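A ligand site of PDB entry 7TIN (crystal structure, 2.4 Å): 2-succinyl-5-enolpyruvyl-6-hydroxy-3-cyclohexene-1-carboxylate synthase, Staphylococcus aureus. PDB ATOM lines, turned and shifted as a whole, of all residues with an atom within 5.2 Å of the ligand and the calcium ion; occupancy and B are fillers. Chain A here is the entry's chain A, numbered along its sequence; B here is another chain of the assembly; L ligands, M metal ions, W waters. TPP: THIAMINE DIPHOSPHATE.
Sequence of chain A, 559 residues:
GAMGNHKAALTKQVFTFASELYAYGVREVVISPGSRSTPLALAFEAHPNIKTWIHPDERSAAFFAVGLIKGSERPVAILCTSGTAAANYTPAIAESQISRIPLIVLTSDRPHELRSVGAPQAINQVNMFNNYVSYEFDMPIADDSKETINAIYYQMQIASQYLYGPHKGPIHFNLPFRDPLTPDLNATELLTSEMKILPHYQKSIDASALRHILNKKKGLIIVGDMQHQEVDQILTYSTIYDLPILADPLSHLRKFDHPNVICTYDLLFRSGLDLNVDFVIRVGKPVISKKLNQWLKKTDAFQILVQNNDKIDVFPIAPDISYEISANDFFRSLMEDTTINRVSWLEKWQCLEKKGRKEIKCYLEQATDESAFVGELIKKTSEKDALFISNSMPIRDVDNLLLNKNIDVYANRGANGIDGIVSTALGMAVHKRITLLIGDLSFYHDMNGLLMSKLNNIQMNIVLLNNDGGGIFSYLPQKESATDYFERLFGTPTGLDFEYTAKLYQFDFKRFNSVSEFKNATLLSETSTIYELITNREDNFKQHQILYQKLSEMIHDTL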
ATOM      1  N   GLU A 370       4.416  16.152  -9.989  1.00  0.00           N
ATOM      2  CA  GLU A 370       4.807  14.959 -10.738  1.00  0.00           C
ATOM      3  C   GLU A 370       4.705  15.179 -12.244  1.00  0.00           C
ATOM      4  O   GLU A 370       5.521  14.641 -13.008  1.00  0.00           O
ATOM      5  CB  GLU A 370       3.946  13.768 -10.314  1.00  0.00           C
ATOM      6  CG  GLU A 370       4.482  12.420 -10.754  1.00  0.00           C
ATOM      7  CD  GLU A 370       3.707  11.244 -10.178  1.00  0.00           C
ATOM      8  OE1 GLU A 370       2.698  10.824 -10.780  1.00  0.00           O
ATOM      9  OE2 GLU A 370       4.103  10.746  -9.094  1.00  0.00           O
ATOM     10  N   SER A 390       4.187   3.173 -17.697  1.00  0.00           N
ATOM     11  CA  SER A 390       3.370   2.349 -16.826  1.00  0.00           C
ATOM     12  C   SER A 390       1.904   2.747 -16.965  1.00  0.00           C
ATOM     13  O   SER A 390       1.543   3.661 -17.705  1.00  0.00           O
ATOM     14  CB  SER A 390       3.857   2.483 -15.379  1.00  0.00           C
ATOM     15  OG  SER A 390       3.218   1.552 -14.534  1.00  0.00           O
ATOM     16  N   ASN A 391       1.043   2.049 -16.233  1.00  0.00           N
ATOM     17  CA  ASN A 391      -0.364   2.442 -16.166  1.00  0.00           C
ATOM     18  C   ASN A 391      -0.539   3.404 -14.985  1.00  0.00           C
ATOM     19  O   ASN A 391       0.447   3.967 -14.492  1.00  0.00           O
ATOM     20  CB  ASN A 391      -1.252   1.196 -16.086  1.00  0.00           C
ATOM     21  CG  ASN A 391      -1.216   0.386 -17.376  1.00  0.00           C
ATOM     22  OD1 ASN A 391      -1.139   0.946 -18.474  1.00  0.00           O
ATOM     23  ND2 ASN A 391      -1.264  -0.930 -17.238  1.00  0.00           N
ATOM     24  N   SER A 392      -1.771   3.606 -14.541  1.00  0.00           N
ATOM     25  CA  SER A 392      -2.095   4.576 -13.482  1.00  0.00           C
ATOM     26  C   SER A 392      -1.750   5.973 -14.009  1.00  0.00           C
ATOM     27  O   SER A 392      -1.925   6.241 -15.212  1.00  0.00           O
ATOM     28  CB  SER A 392      -1.406   4.188 -12.187  1.00  0.00           C
ATOM     29  OG  SER A 392      -2.110   4.698 -11.065  1.00  0.00           O
ATOM     30  N   MET A 393      -1.266   6.891 -13.164  1.00  0.00           N
ATOM     31  CA  MET A 393      -1.085   8.277 -13.570  1.00  0.00           C
ATOM     32  C   MET A 393      -0.112   8.494 -14.729  1.00  0.00           C
ATOM     33  O   MET A 393      -0.407   9.357 -15.581  1.00  0.00           O
ATOM     34  CB  MET A 393      -0.655   9.125 -12.370  1.00  0.00           C
ATOM     35  CG  MET A 393      -1.800   9.537 -11.452  1.00  0.00           C
ATOM     36  SD  MET A 393      -3.390   9.702 -12.304  1.00  0.00           S
ATOM     37  CE  MET A 393      -3.270  11.333 -13.017  1.00  0.00           C
ATOM     38  N   PRO A 394       1.036   7.807 -14.827  1.00  0.00           N
ATOM     39  CA  PRO A 394       1.997   8.136 -15.903  1.00  0.00           C
ATOM     40  C   PRO A 394       1.400   8.104 -17.300  1.00  0.00           C
ATOM     41  O   PRO A 394       1.701   8.993 -18.107  1.00  0.00           O
ATOM     42  CB  PRO A 394       3.083   7.085 -15.726  1.00  0.00           C
ATOM     43  CG  PRO A 394       3.092   6.821 -14.272  1.00  0.00           C
ATOM     44  CD  PRO A 394       1.643   6.864 -13.857  1.00  0.00           C
ATOM     45  N   ASN A 416      -4.785  -3.150 -18.481  1.00  0.00           N
ATOM     46  CA  ASN A 416      -4.402  -2.001 -17.663  1.00  0.00           C
ATOM     47  C   ASN A 416      -3.928  -2.431 -16.284  1.00  0.00           C
ATOM     48  O   ASN A 416      -4.309  -1.855 -15.254  1.00  0.00           O
ATOM     49  CB  ASN A 416      -5.552  -0.999 -17.562  1.00  0.00           C
ATOM     50  CG  ASN A 416      -6.025  -0.519 -18.928  1.00  0.00           C
ATOM     51  OD1 ASN A 416      -5.275  -0.545 -19.903  1.00  0.00           O
ATOM     52  ND2 ASN A 416      -7.271  -0.070 -18.991  1.00  0.00           N
ATOM     53  N   GLY A 417      -3.099  -3.470 -16.244  1.00  0.00           N
ATOM     54  CA  GLY A 417      -2.590  -3.972 -14.997  1.00  0.00           C
ATOM     55  C   GLY A 417      -1.343  -3.213 -14.539  1.00  0.00           C
ATOM     56  O   GLY A 417      -0.606  -2.657 -15.339  1.00  0.00           O
ATOM     57  N   ILE A 418      -1.138  -3.213 -13.216  1.00  0.00           N
ATOM     58  CA  ILE A 418       0.101  -2.696 -12.656  1.00  0.00           C
ATOM     59  C   ILE A 418       1.130  -3.795 -12.456  1.00  0.00           C
ATOM     60  O   ILE A 418       2.226  -3.537 -11.935  1.00  0.00           O
ATOM     61  CB  ILE A 418      -0.155  -1.974 -11.314  1.00  0.00           C
ATOM     62  CG1 ILE A 418      -0.612  -2.984 -10.257  1.00  0.00           C
ATOM     63  CG2 ILE A 418      -1.166  -0.853 -11.503  1.00  0.00           C
ATOM     64  CD1 ILE A 418      -1.020  -2.347  -8.942  1.00  0.00           C
ATOM     65  N   ASP A 419       0.820  -5.028 -12.858  1.00  0.00           N
ATOM     66  CA  ASP A 419       1.744  -6.145 -12.743  1.00  0.00           C
ATOM     67  C   ASP A 419       2.552  -6.294 -14.025  1.00  0.00           C
ATOM     68  O   ASP A 419       2.101  -5.962 -15.115  1.00  0.00           O
ATOM     69  CB  ASP A 419       0.991  -7.448 -12.446  1.00  0.00           C
ATOM     70  CG  ASP A 419      -0.307  -7.583 -13.238  1.00  0.00           C
ATOM     71  OD1 ASP A 419      -0.665  -6.660 -14.008  1.00  0.00           O
ATOM     72  OD2 ASP A 419      -0.980  -8.629 -13.088  1.00  0.00           O
ATOM     73  N   GLY A 439       5.329   4.099 -11.697  1.00  0.00           N
ATOM     74  CA  GLY A 439       5.046   4.470 -10.328  1.00  0.00           C
ATOM     75  C   GLY A 439       5.556   3.435  -9.325  1.00  0.00           C
ATOM     76  O   GLY A 439       5.936   2.320  -9.683  1.00  0.00           O
ATOM     77  N   ASP A 440       5.563   3.834  -8.049  1.00  0.00           N
ATOM     78  CA  ASP A 440       6.242   3.018  -7.034  1.00  0.00           C
ATOM     79  C   ASP A 440       5.495   1.714  -6.770  1.00  0.00           C
ATOM     80  O   ASP A 440       6.125   0.673  -6.557  1.00  0.00           O
ATOM     81  CB  ASP A 440       6.418   3.814  -5.744  1.00  0.00           C
ATOM     82  CG  ASP A 440       5.145   4.530  -5.314  1.00  0.00           C
ATOM     83  OD1 ASP A 440       4.779   5.518  -5.983  1.00  0.00           O
ATOM     84  OD2 ASP A 440       4.528   4.108  -4.310  1.00  0.00           O
ATOM     85  N   LEU A 441       4.164   1.738  -6.767  1.00  0.00           N
ATOM     86  CA  LEU A 441       3.421   0.514  -6.485  1.00  0.00           C
ATOM     87  C   LEU A 441       3.616  -0.518  -7.591  1.00  0.00           C
ATOM     88  O   LEU A 441       3.814  -1.702  -7.310  1.00  0.00           O
ATOM     89  CB  LEU A 441       1.938   0.817  -6.263  1.00  0.00           C
ATOM     90  CG  LEU A 441       1.587   1.492  -4.931  1.00  0.00           C
ATOM     91  CD1 LEU A 441       0.082   1.662  -4.777  1.00  0.00           C
ATOM     92  CD2 LEU A 441       2.161   0.722  -3.742  1.00  0.00           C
ATOM     93  N   SER A 442       3.589  -0.087  -8.863  1.00  0.00           N
ATOM     94  CA  SER A 442       3.891  -1.024  -9.941  1.00  0.00           C
ATOM     95  C   SER A 442       5.353  -1.444  -9.912  1.00  0.00           C
ATOM     96  O   SER A 442       5.675  -2.592 -10.232  1.00  0.00           O
ATOM     97  CB  SER A 442       3.529  -0.439 -11.308  1.00  0.00           C
ATOM     98  OG  SER A 442       2.831   0.780 -11.188  1.00  0.00           O
ATOM     99  N   HIS A 445       5.415  -4.082  -7.542  1.00  0.00           N
ATOM    100  CA  HIS A 445       4.697  -5.269  -8.006  1.00  0.00           C
ATOM    101  C   HIS A 445       5.623  -6.219  -8.769  1.00  0.00           C
ATOM    102  O   HIS A 445       5.653  -7.419  -8.506  1.00  0.00           O
ATOM    103  CB  HIS A 445       3.505  -4.856  -8.871  1.00  0.00           C
ATOM    104  CG  HIS A 445       2.285  -5.698  -8.648  1.00  0.00           C
ATOM    105  ND1 HIS A 445       2.109  -6.935  -9.242  1.00  0.00           N
ATOM    106  CD2 HIS A 445       1.175  -5.482  -7.912  1.00  0.00           C
ATOM    107  CE1 HIS A 445       0.948  -7.437  -8.877  1.00  0.00           C
ATOM    108  NE2 HIS A 445       0.355  -6.575  -8.066  1.00  0.00           N
ATOM    109  N   LEU A 465       8.798   7.242 -10.389  1.00  0.00           N
ATOM    110  CA  LEU A 465       7.969   8.259  -9.759  1.00  0.00           C
ATOM    111  C   LEU A 465       7.440   7.693  -8.451  1.00  0.00           C
ATOM    112  O   LEU A 465       6.538   6.838  -8.455  1.00  0.00           O
ATOM    113  CB  LEU A 465       6.827   8.686 -10.674  1.00  0.00           C
ATOM    114  CG  LEU A 465       7.221   9.400 -11.957  1.00  0.00           C
ATOM    115  CD1 LEU A 465       5.986   9.776 -12.757  1.00  0.00           C
ATOM    116  CD2 LEU A 465       8.068  10.624 -11.652  1.00  0.00           C
ATOM    117  N   ASN A 467       5.566   8.556  -5.111  1.00  0.00           N
ATOM    118  CA  ASN A 467       4.772   9.366  -4.212  1.00  0.00           C
ATOM    119  C   ASN A 467       4.227   8.541  -3.047  1.00  0.00           C
ATOM    120  O   ASN A 467       3.284   8.975  -2.372  1.00  0.00           O
ATOM    121  CB  ASN A 467       3.647  10.065  -4.961  1.00  0.00           C
ATOM    122  CG  ASN A 467       2.845   9.132  -5.850  1.00  0.00           C
ATOM    123  OD1 ASN A 467       2.425   8.057  -5.429  1.00  0.00           O
ATOM    124  ND2 ASN A 467       2.639   9.543  -7.096  1.00  0.00           N
ATOM    125  N   ASP A 468       4.790   7.357  -2.821  1.00  0.00           N
ATOM    126  CA  ASP A 468       4.458   6.495  -1.683  1.00  0.00           C
ATOM    127  C   ASP A 468       2.952   6.229  -1.593  1.00  0.00           C
ATOM    128  O   ASP A 468       2.268   6.647  -0.655  1.00  0.00           O
ATOM    129  CB  ASP A 468       4.993   7.104  -0.387  1.00  0.00           C
ATOM    130  CG  ASP A 468       5.266   6.059   0.680  1.00  0.00           C
ATOM    131  OD1 ASP A 468       5.544   4.892   0.324  1.00  0.00           O
ATOM    132  OD2 ASP A 468       5.192   6.399   1.887  1.00  0.00           O
ATOM    133  N   GLY A 469       2.454   5.520  -2.585  1.00  0.00           N
ATOM    134  CA  GLY A 469       1.086   5.084  -2.588  1.00  0.00           C
ATOM    135  C   GLY A 469       0.473   5.173  -3.973  1.00  0.00           C
ATOM    136  O   GLY A 469       1.175   5.334  -4.966  1.00  0.00           O
ATOM    137  N   GLY A 470      -0.854   5.062  -4.014  1.00  0.00           N
ATOM    138  CA  GLY A 470      -1.580   5.113  -5.266  1.00  0.00           C
ATOM    139  C   GLY A 470      -2.194   6.471  -5.543  1.00  0.00           C
ATOM    140  O   GLY A 470      -3.299   6.774  -5.073  1.00  0.00           O
ATOM    141  N   GLY A 471      -1.476   7.301  -6.315  1.00  0.00           N
ATOM    142  CA  GLY A 471      -1.922   8.661  -6.527  1.00  0.00           C
ATOM    143  C   GLY A 471      -3.203   8.788  -7.334  1.00  0.00           C
ATOM    144  O   GLY A 471      -3.959   9.734  -7.150  1.00  0.00           O
ATOM    145  N   ILE A 472      -3.461   7.835  -8.241  1.00  0.00           N
ATOM    146  CA  ILE A 472      -4.628   7.925  -9.104  1.00  0.00           C
ATOM    147  C   ILE A 472      -5.915   7.973  -8.304  1.00  0.00           C
ATOM    148  O   ILE A 472      -6.923   8.535  -8.754  1.00  0.00           O
ATOM    149  CB  ILE A 472      -4.635   6.756 -10.122  1.00  0.00           C
ATOM    150  CG1 ILE A 472      -5.615   7.042 -11.257  1.00  0.00           C
ATOM    151  CG2 ILE A 472      -4.989   5.428  -9.440  1.00  0.00           C
ATOM    152  CD1 ILE A 472      -5.242   6.377 -12.571  1.00  0.00           C
ATOM    153  N   PHE A 473      -5.918   7.405  -7.089  1.00  0.00           N
ATOM    154  CA  PHE A 473      -7.146   7.372  -6.301  1.00  0.00           C
ATOM    155  C   PHE A 473      -7.455   8.715  -5.652  1.00  0.00           C
ATOM    156  O   PHE A 473      -8.552   8.870  -5.103  1.00  0.00           O
ATOM    157  CB  PHE A 473      -7.061   6.274  -5.244  1.00  0.00           C
ATOM    158  CG  PHE A 473      -6.838   4.907  -5.826  1.00  0.00           C
ATOM    159  CD1 PHE A 473      -7.680   4.417  -6.811  1.00  0.00           C
ATOM    160  CD2 PHE A 473      -5.774   4.123  -5.411  1.00  0.00           C
ATOM    161  CE1 PHE A 473      -7.469   3.166  -7.362  1.00  0.00           C
ATOM    162  CE2 PHE A 473      -5.570   2.867  -5.951  1.00  0.00           C
ATOM    163  CZ  PHE A 473      -6.413   2.386  -6.933  1.00  0.00           C
ATOM    164  N   PRO B  33      -5.837  -3.096  -3.142  1.00  0.00           N
ATOM    165  CA  PRO B  33      -6.391  -1.798  -3.575  1.00  0.00           C
ATOM    166  C   PRO B  33      -6.951  -1.861  -4.988  1.00  0.00           C
ATOM    167  O   PRO B  33      -6.406  -2.532  -5.869  1.00  0.00           O
ATOM    168  CB  PRO B  33      -5.181  -0.863  -3.499  1.00  0.00           C
ATOM    169  CG  PRO B  33      -3.992  -1.764  -3.595  1.00  0.00           C
ATOM    170  CD  PRO B  33      -4.391  -3.021  -2.895  1.00  0.00           C
ATOM    171  N   GLY B  34      -8.056  -1.145  -5.189  1.00  0.00           N
ATOM    172  CA  GLY B  34      -8.666  -1.013  -6.501  1.00  0.00           C
ATOM    173  C   GLY B  34      -9.897  -0.137  -6.380  1.00  0.00           C
ATOM    174  O   GLY B  34     -10.418   0.110  -5.290  1.00  0.00           O
ATOM    175  N   GLU B  58      -1.420  -9.017  -5.258  1.00  0.00           N
ATOM    176  CA  GLU B  58      -2.484 -10.000  -5.106  1.00  0.00           C
ATOM    177  C   GLU B  58      -1.928 -11.423  -5.010  1.00  0.00           C
ATOM    178  O   GLU B  58      -2.450 -12.247  -4.240  1.00  0.00           O
ATOM    179  CB  GLU B  58      -3.477  -9.890  -6.259  1.00  0.00           C
ATOM    180  CG  GLU B  58      -4.329  -8.636  -6.253  1.00  0.00           C
ATOM    181  CD  GLU B  58      -3.648  -7.449  -6.931  1.00  0.00           C
ATOM    182  OE1 GLU B  58      -2.493  -7.592  -7.375  1.00  0.00           O
ATOM    183  OE2 GLU B  58      -4.276  -6.369  -7.019  1.00  0.00           O
ATOM    184  N   THR B  81      -9.899  -5.987  -7.025  1.00  0.00           N
ATOM    185  CA  THR B  81     -10.612  -5.265  -8.066  1.00  0.00           C
ATOM    186  C   THR B  81     -10.626  -6.083  -9.356  1.00  0.00           C
ATOM    187  O   THR B  81     -10.021  -7.158  -9.451  1.00  0.00           O
ATOM    188  CB  THR B  81      -9.964  -3.891  -8.268  1.00  0.00           C
ATOM    189  OG1 THR B  81     -10.852  -3.036  -9.003  1.00  0.00           O
ATOM    190  CG2 THR B  81      -8.632  -4.026  -8.995  1.00  0.00           C
ATOM    191  N   THR B  84      -6.645  -8.215 -14.163  1.00  0.00           N
ATOM    192  CA  THR B  84      -5.556  -9.135 -13.850  1.00  0.00           C
ATOM    193  C   THR B  84      -5.284  -9.244 -12.357  1.00  0.00           C
ATOM    194  O   THR B  84      -4.529 -10.145 -11.961  1.00  0.00           O
ATOM    195  CB  THR B  84      -4.256  -8.722 -14.553  1.00  0.00           C
ATOM    196  OG1 THR B  84      -3.993  -7.326 -14.311  1.00  0.00           O
ATOM    197  CG2 THR B  84      -4.361  -8.970 -16.054  1.00  0.00           C
ATOM    198  N   ALA B  85      -5.842  -8.354 -11.547  1.00  0.00           N
ATOM    199  CA  ALA B  85      -5.761  -8.529 -10.100  1.00  0.00           C
ATOM    200  C   ALA B  85      -6.279  -9.896  -9.684  1.00  0.00           C
ATOM    201  O   ALA B  85      -5.645 -10.590  -8.871  1.00  0.00           O
ATOM    202  CB  ALA B  85      -6.557  -7.422  -9.393  1.00  0.00           C
ATOM    203  N   ASN B  88      -3.942 -12.941 -10.660  1.00  0.00           N
ATOM    204  CA  ASN B  88      -2.849 -13.199  -9.735  1.00  0.00           C
ATOM    205  C   ASN B  88      -3.238 -14.110  -8.575  1.00  0.00           C
ATOM    206  O   ASN B  88      -2.349 -14.605  -7.880  1.00  0.00           O
ATOM    207  CB  ASN B  88      -2.302 -11.881  -9.178  1.00  0.00           C
ATOM    208  CG  ASN B  88      -1.443 -11.125 -10.191  1.00  0.00           C
ATOM    209  OD1 ASN B  88      -0.236 -11.350 -10.277  1.00  0.00           O
ATOM    210  ND2 ASN B  88      -2.062 -10.226 -10.937  1.00  0.00           N
ATOM    211  N   GLN B 121      -9.599  -3.564 -19.461  1.00  0.00           N
ATOM    212  CA  GLN B 121      -9.563  -4.167 -18.137  1.00  0.00           C
ATOM    213  C   GLN B 121     -10.711  -5.148 -17.933  1.00  0.00           C
ATOM    214  O   GLN B 121     -11.150  -5.394 -16.802  1.00  0.00           O
ATOM    215  CB  GLN B 121      -9.579  -3.100 -17.032  1.00  0.00           C
ATOM    216  CG  GLN B 121      -8.987  -3.536 -15.705  1.00  0.00           C
ATOM    217  CD  GLN B 121      -8.821  -2.382 -14.749  1.00  0.00           C
ATOM    218  OE1 GLN B 121      -8.151  -1.396 -15.060  1.00  0.00           O
ATOM    219  NE2 GLN B 121      -9.430  -2.492 -13.577  1.00  0.00           N
HETATM  220  N1' TPP L   1      -4.046  -4.754  -9.239  1.00  0.00           N
HETATM  221  C2' TPP L   1      -3.568  -4.856 -10.494  1.00  0.00           C
HETATM  222  CM2 TPP L   1      -2.801  -6.094 -10.836  1.00  0.00           C
HETATM  223  N3' TPP L   1      -3.707  -3.943 -11.456  1.00  0.00           N
HETATM  224  C4' TPP L   1      -4.391  -2.824 -11.163  1.00  0.00           C
HETATM  225  N4' TPP L   1      -4.522  -1.923 -12.150  1.00  0.00           N
HETATM  226  C5' TPP L   1      -4.939  -2.619  -9.866  1.00  0.00           C
HETATM  227  C6' TPP L   1      -4.725  -3.628  -8.966  1.00  0.00           C
HETATM  228  C7' TPP L   1      -5.710  -1.374  -9.480  1.00  0.00           C
HETATM  229  N3  TPP L   1      -4.914  -0.130  -9.611  1.00  0.00           N
HETATM  230  C2  TPP L   1      -4.991   0.680 -10.654  1.00  0.00           C
HETATM  231  S1  TPP L   1      -3.943   1.982 -10.525  1.00  0.00           S
HETATM  232  C5  TPP L   1      -3.377   1.418  -8.990  1.00  0.00           C
HETATM  233  C4  TPP L   1      -3.991   0.265  -8.647  1.00  0.00           C
HETATM  234  CM4 TPP L   1      -3.786  -0.544  -7.413  1.00  0.00           C
HETATM  235  C6  TPP L   1      -2.328   2.181  -8.231  1.00  0.00           C
HETATM  236  C7  TPP L   1      -0.944   2.045  -8.843  1.00  0.00           C
HETATM  237  O7  TPP L   1      -0.066   2.999  -8.199  1.00  0.00           O
HETATM  238  PA  TPP L   1       1.313   3.469  -8.791  1.00  0.00           P
HETATM  239  O1A TPP L   1       2.248   3.788  -7.626  1.00  0.00           O
HETATM  240  O2A TPP L   1       1.850   2.497  -9.774  1.00  0.00           O
HETATM  241  O3A TPP L   1       0.949   4.831  -9.475  1.00  0.00           O
HETATM  242  PB  TPP L   1       0.143   6.166  -9.165  1.00  0.00           P
HETATM  243  O1B TPP L   1       0.796   6.733  -7.906  1.00  0.00           O
HETATM  244  O2B TPP L   1       0.468   7.069 -10.344  1.00  0.00           O
HETATM  245  O3B TPP L   1      -1.316   5.895  -8.991  1.00  0.00           O
HETATM  246 CA    CA M   1       2.591   6.014  -6.645  1.00  0.00          CA
HETATM  247  O   HOH W   1      -2.962  -3.868  -6.253  1.00  0.00           O
HETATM  248  O   HOH W   2       3.685   6.985  -8.516  1.00  0.00           O
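The backbone NH of Asp 440 lies close to an oxygen (O1A) of the ligand, 3.3 Å away. An oxygen (O2A) of the ligand lies within hydrogen-bond range of the backbone NH (N) of Ser 442 (3.2 Å). OG of Ser 442 sits at hydrogen-bond distance from O2A of the ligand (2.4 Å). O3B of the ligand is in hydrogen-bond range of OG of Ser 392 (2.5 Å). N1' of the ligand sits at hydrogen-bond distance from OE2 of Glu 58 of chain B. N of Gly 471 is in hydrogen-bond range of O3B of the ligand (3.0 Å). N of Leu 441 sits close to O1A of the ligand (2.9 Å). An oxygen (O3B) of the ligand is in hydrogen-bond range of the backbone NH (N) of Ile 472 (3.0 Å). The backbone NH of Met 393 lies close to an oxygen (O2B) of the ligand, at 3.3 Å. A nitrogen (N4') of the ligand sits at hydrogen-bond distance from the backbone carbonyl oxygen (O) of Asn 416 (3.1 Å). The backbone NH (N) of Ile 418 lies within hydrogen-bond range of a nitrogen (N3') of the ligand, at 3.2 Å.
The backbone carbonyl oxygen of Leu 465 is in hydrogen-bond range of the backbone NH of Asp 440. ND2 of Asn 467 lies within hydrogen-bond range of OE2 of Glu 370. OG of Ser 390 sits at hydrogen-bond distance from OG of Ser 442, 3.5 Å away. The side-chain carboxylate (OE1) of Glu 58 of chain B is in hydrogen-bond range of a ring nitrogen (NE2) of His 445, 3.1 Å away. The side-chain amide nitrogen (ND2) of Asn 391 sits at hydrogen-bond distance from the backbone carbonyl oxygen (O) of Gly 417, at 2.6 Å. OD1 of Asp 419 lies within hydrogen-bond range of OG1 of Thr 84 of chain B. The side-chain amide nitrogen (ND2) of Asn 88 of chain B sits at hydrogen-bond distance from the side-chain carboxylate (OD2) of Asp 419, at 2.9 Å. The backbone carbonyl oxygen (O) of Thr 84 of chain B is in hydrogen-bond range of the side-chain amide nitrogen (ND2) of Asn 88 of chain B, at 2.7 Å.
Pro 394 touches the ligand. CA of Gly 417 touches N3' of the ligand (3.7 Å). Asp 419 touches the ligand (CG to CM2, 3.8 Å). Gly 439 touches the ligand. Gly 470 touches the ligand. Phe 473 touches the ligand (CZ to C4, 3.6 Å). Pro 33 of chain B touches the ligand. Thr 81 of chain B touches the ligand (CG2 to C6', 3.9 Å). Thr 84 of chain B touches the ligand. Ala 85 of chain B touches the ligand. Hydrophobic or aromatic side chains that line the ligand: Met 393, Pro 394, Ile 418, Leu 441, Ile 472, Phe 473 and Ala 85 of chain B. Within 4 Å of the ligand: Ser 392, Met 393, Pro 394, Asn 416, Gly 417, Ile 418, Asp 419, Gly 439, Asp 440, Leu 441, Ser 442, Asn 467, Gly 469, Gly 470, Gly 471, Ile 472, Phe 473, Pro 33 of chain B, Glu 58 of chain B, Thr 81 of chain B, Thr 84 of chain B and Ala 85 of chain B.
The calcium ion is bound by O of Gly 469 (2.3 Å). The calcium ion is bound by O1B of the ligand. OD1 of Asp 440 binds the calcium ion (2.3 Å). Water W2 binds the calcium ion. The calcium ion is bound by OD1 of Asn 467, 2.4 Å away. O1A of the ligand is bound to the calcium ion, 2.5 Å away.
Water W2 bridges O of Leu 465 (2.9 Å) and ND2 of Asn 467 (3.1 Å). Water W1 lies within hydrogen-bond range of the side-chain carboxylate of Glu 58 of chain B (2.9 Å) and a nitrogen (N1') of the ligand (3.3 Å).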
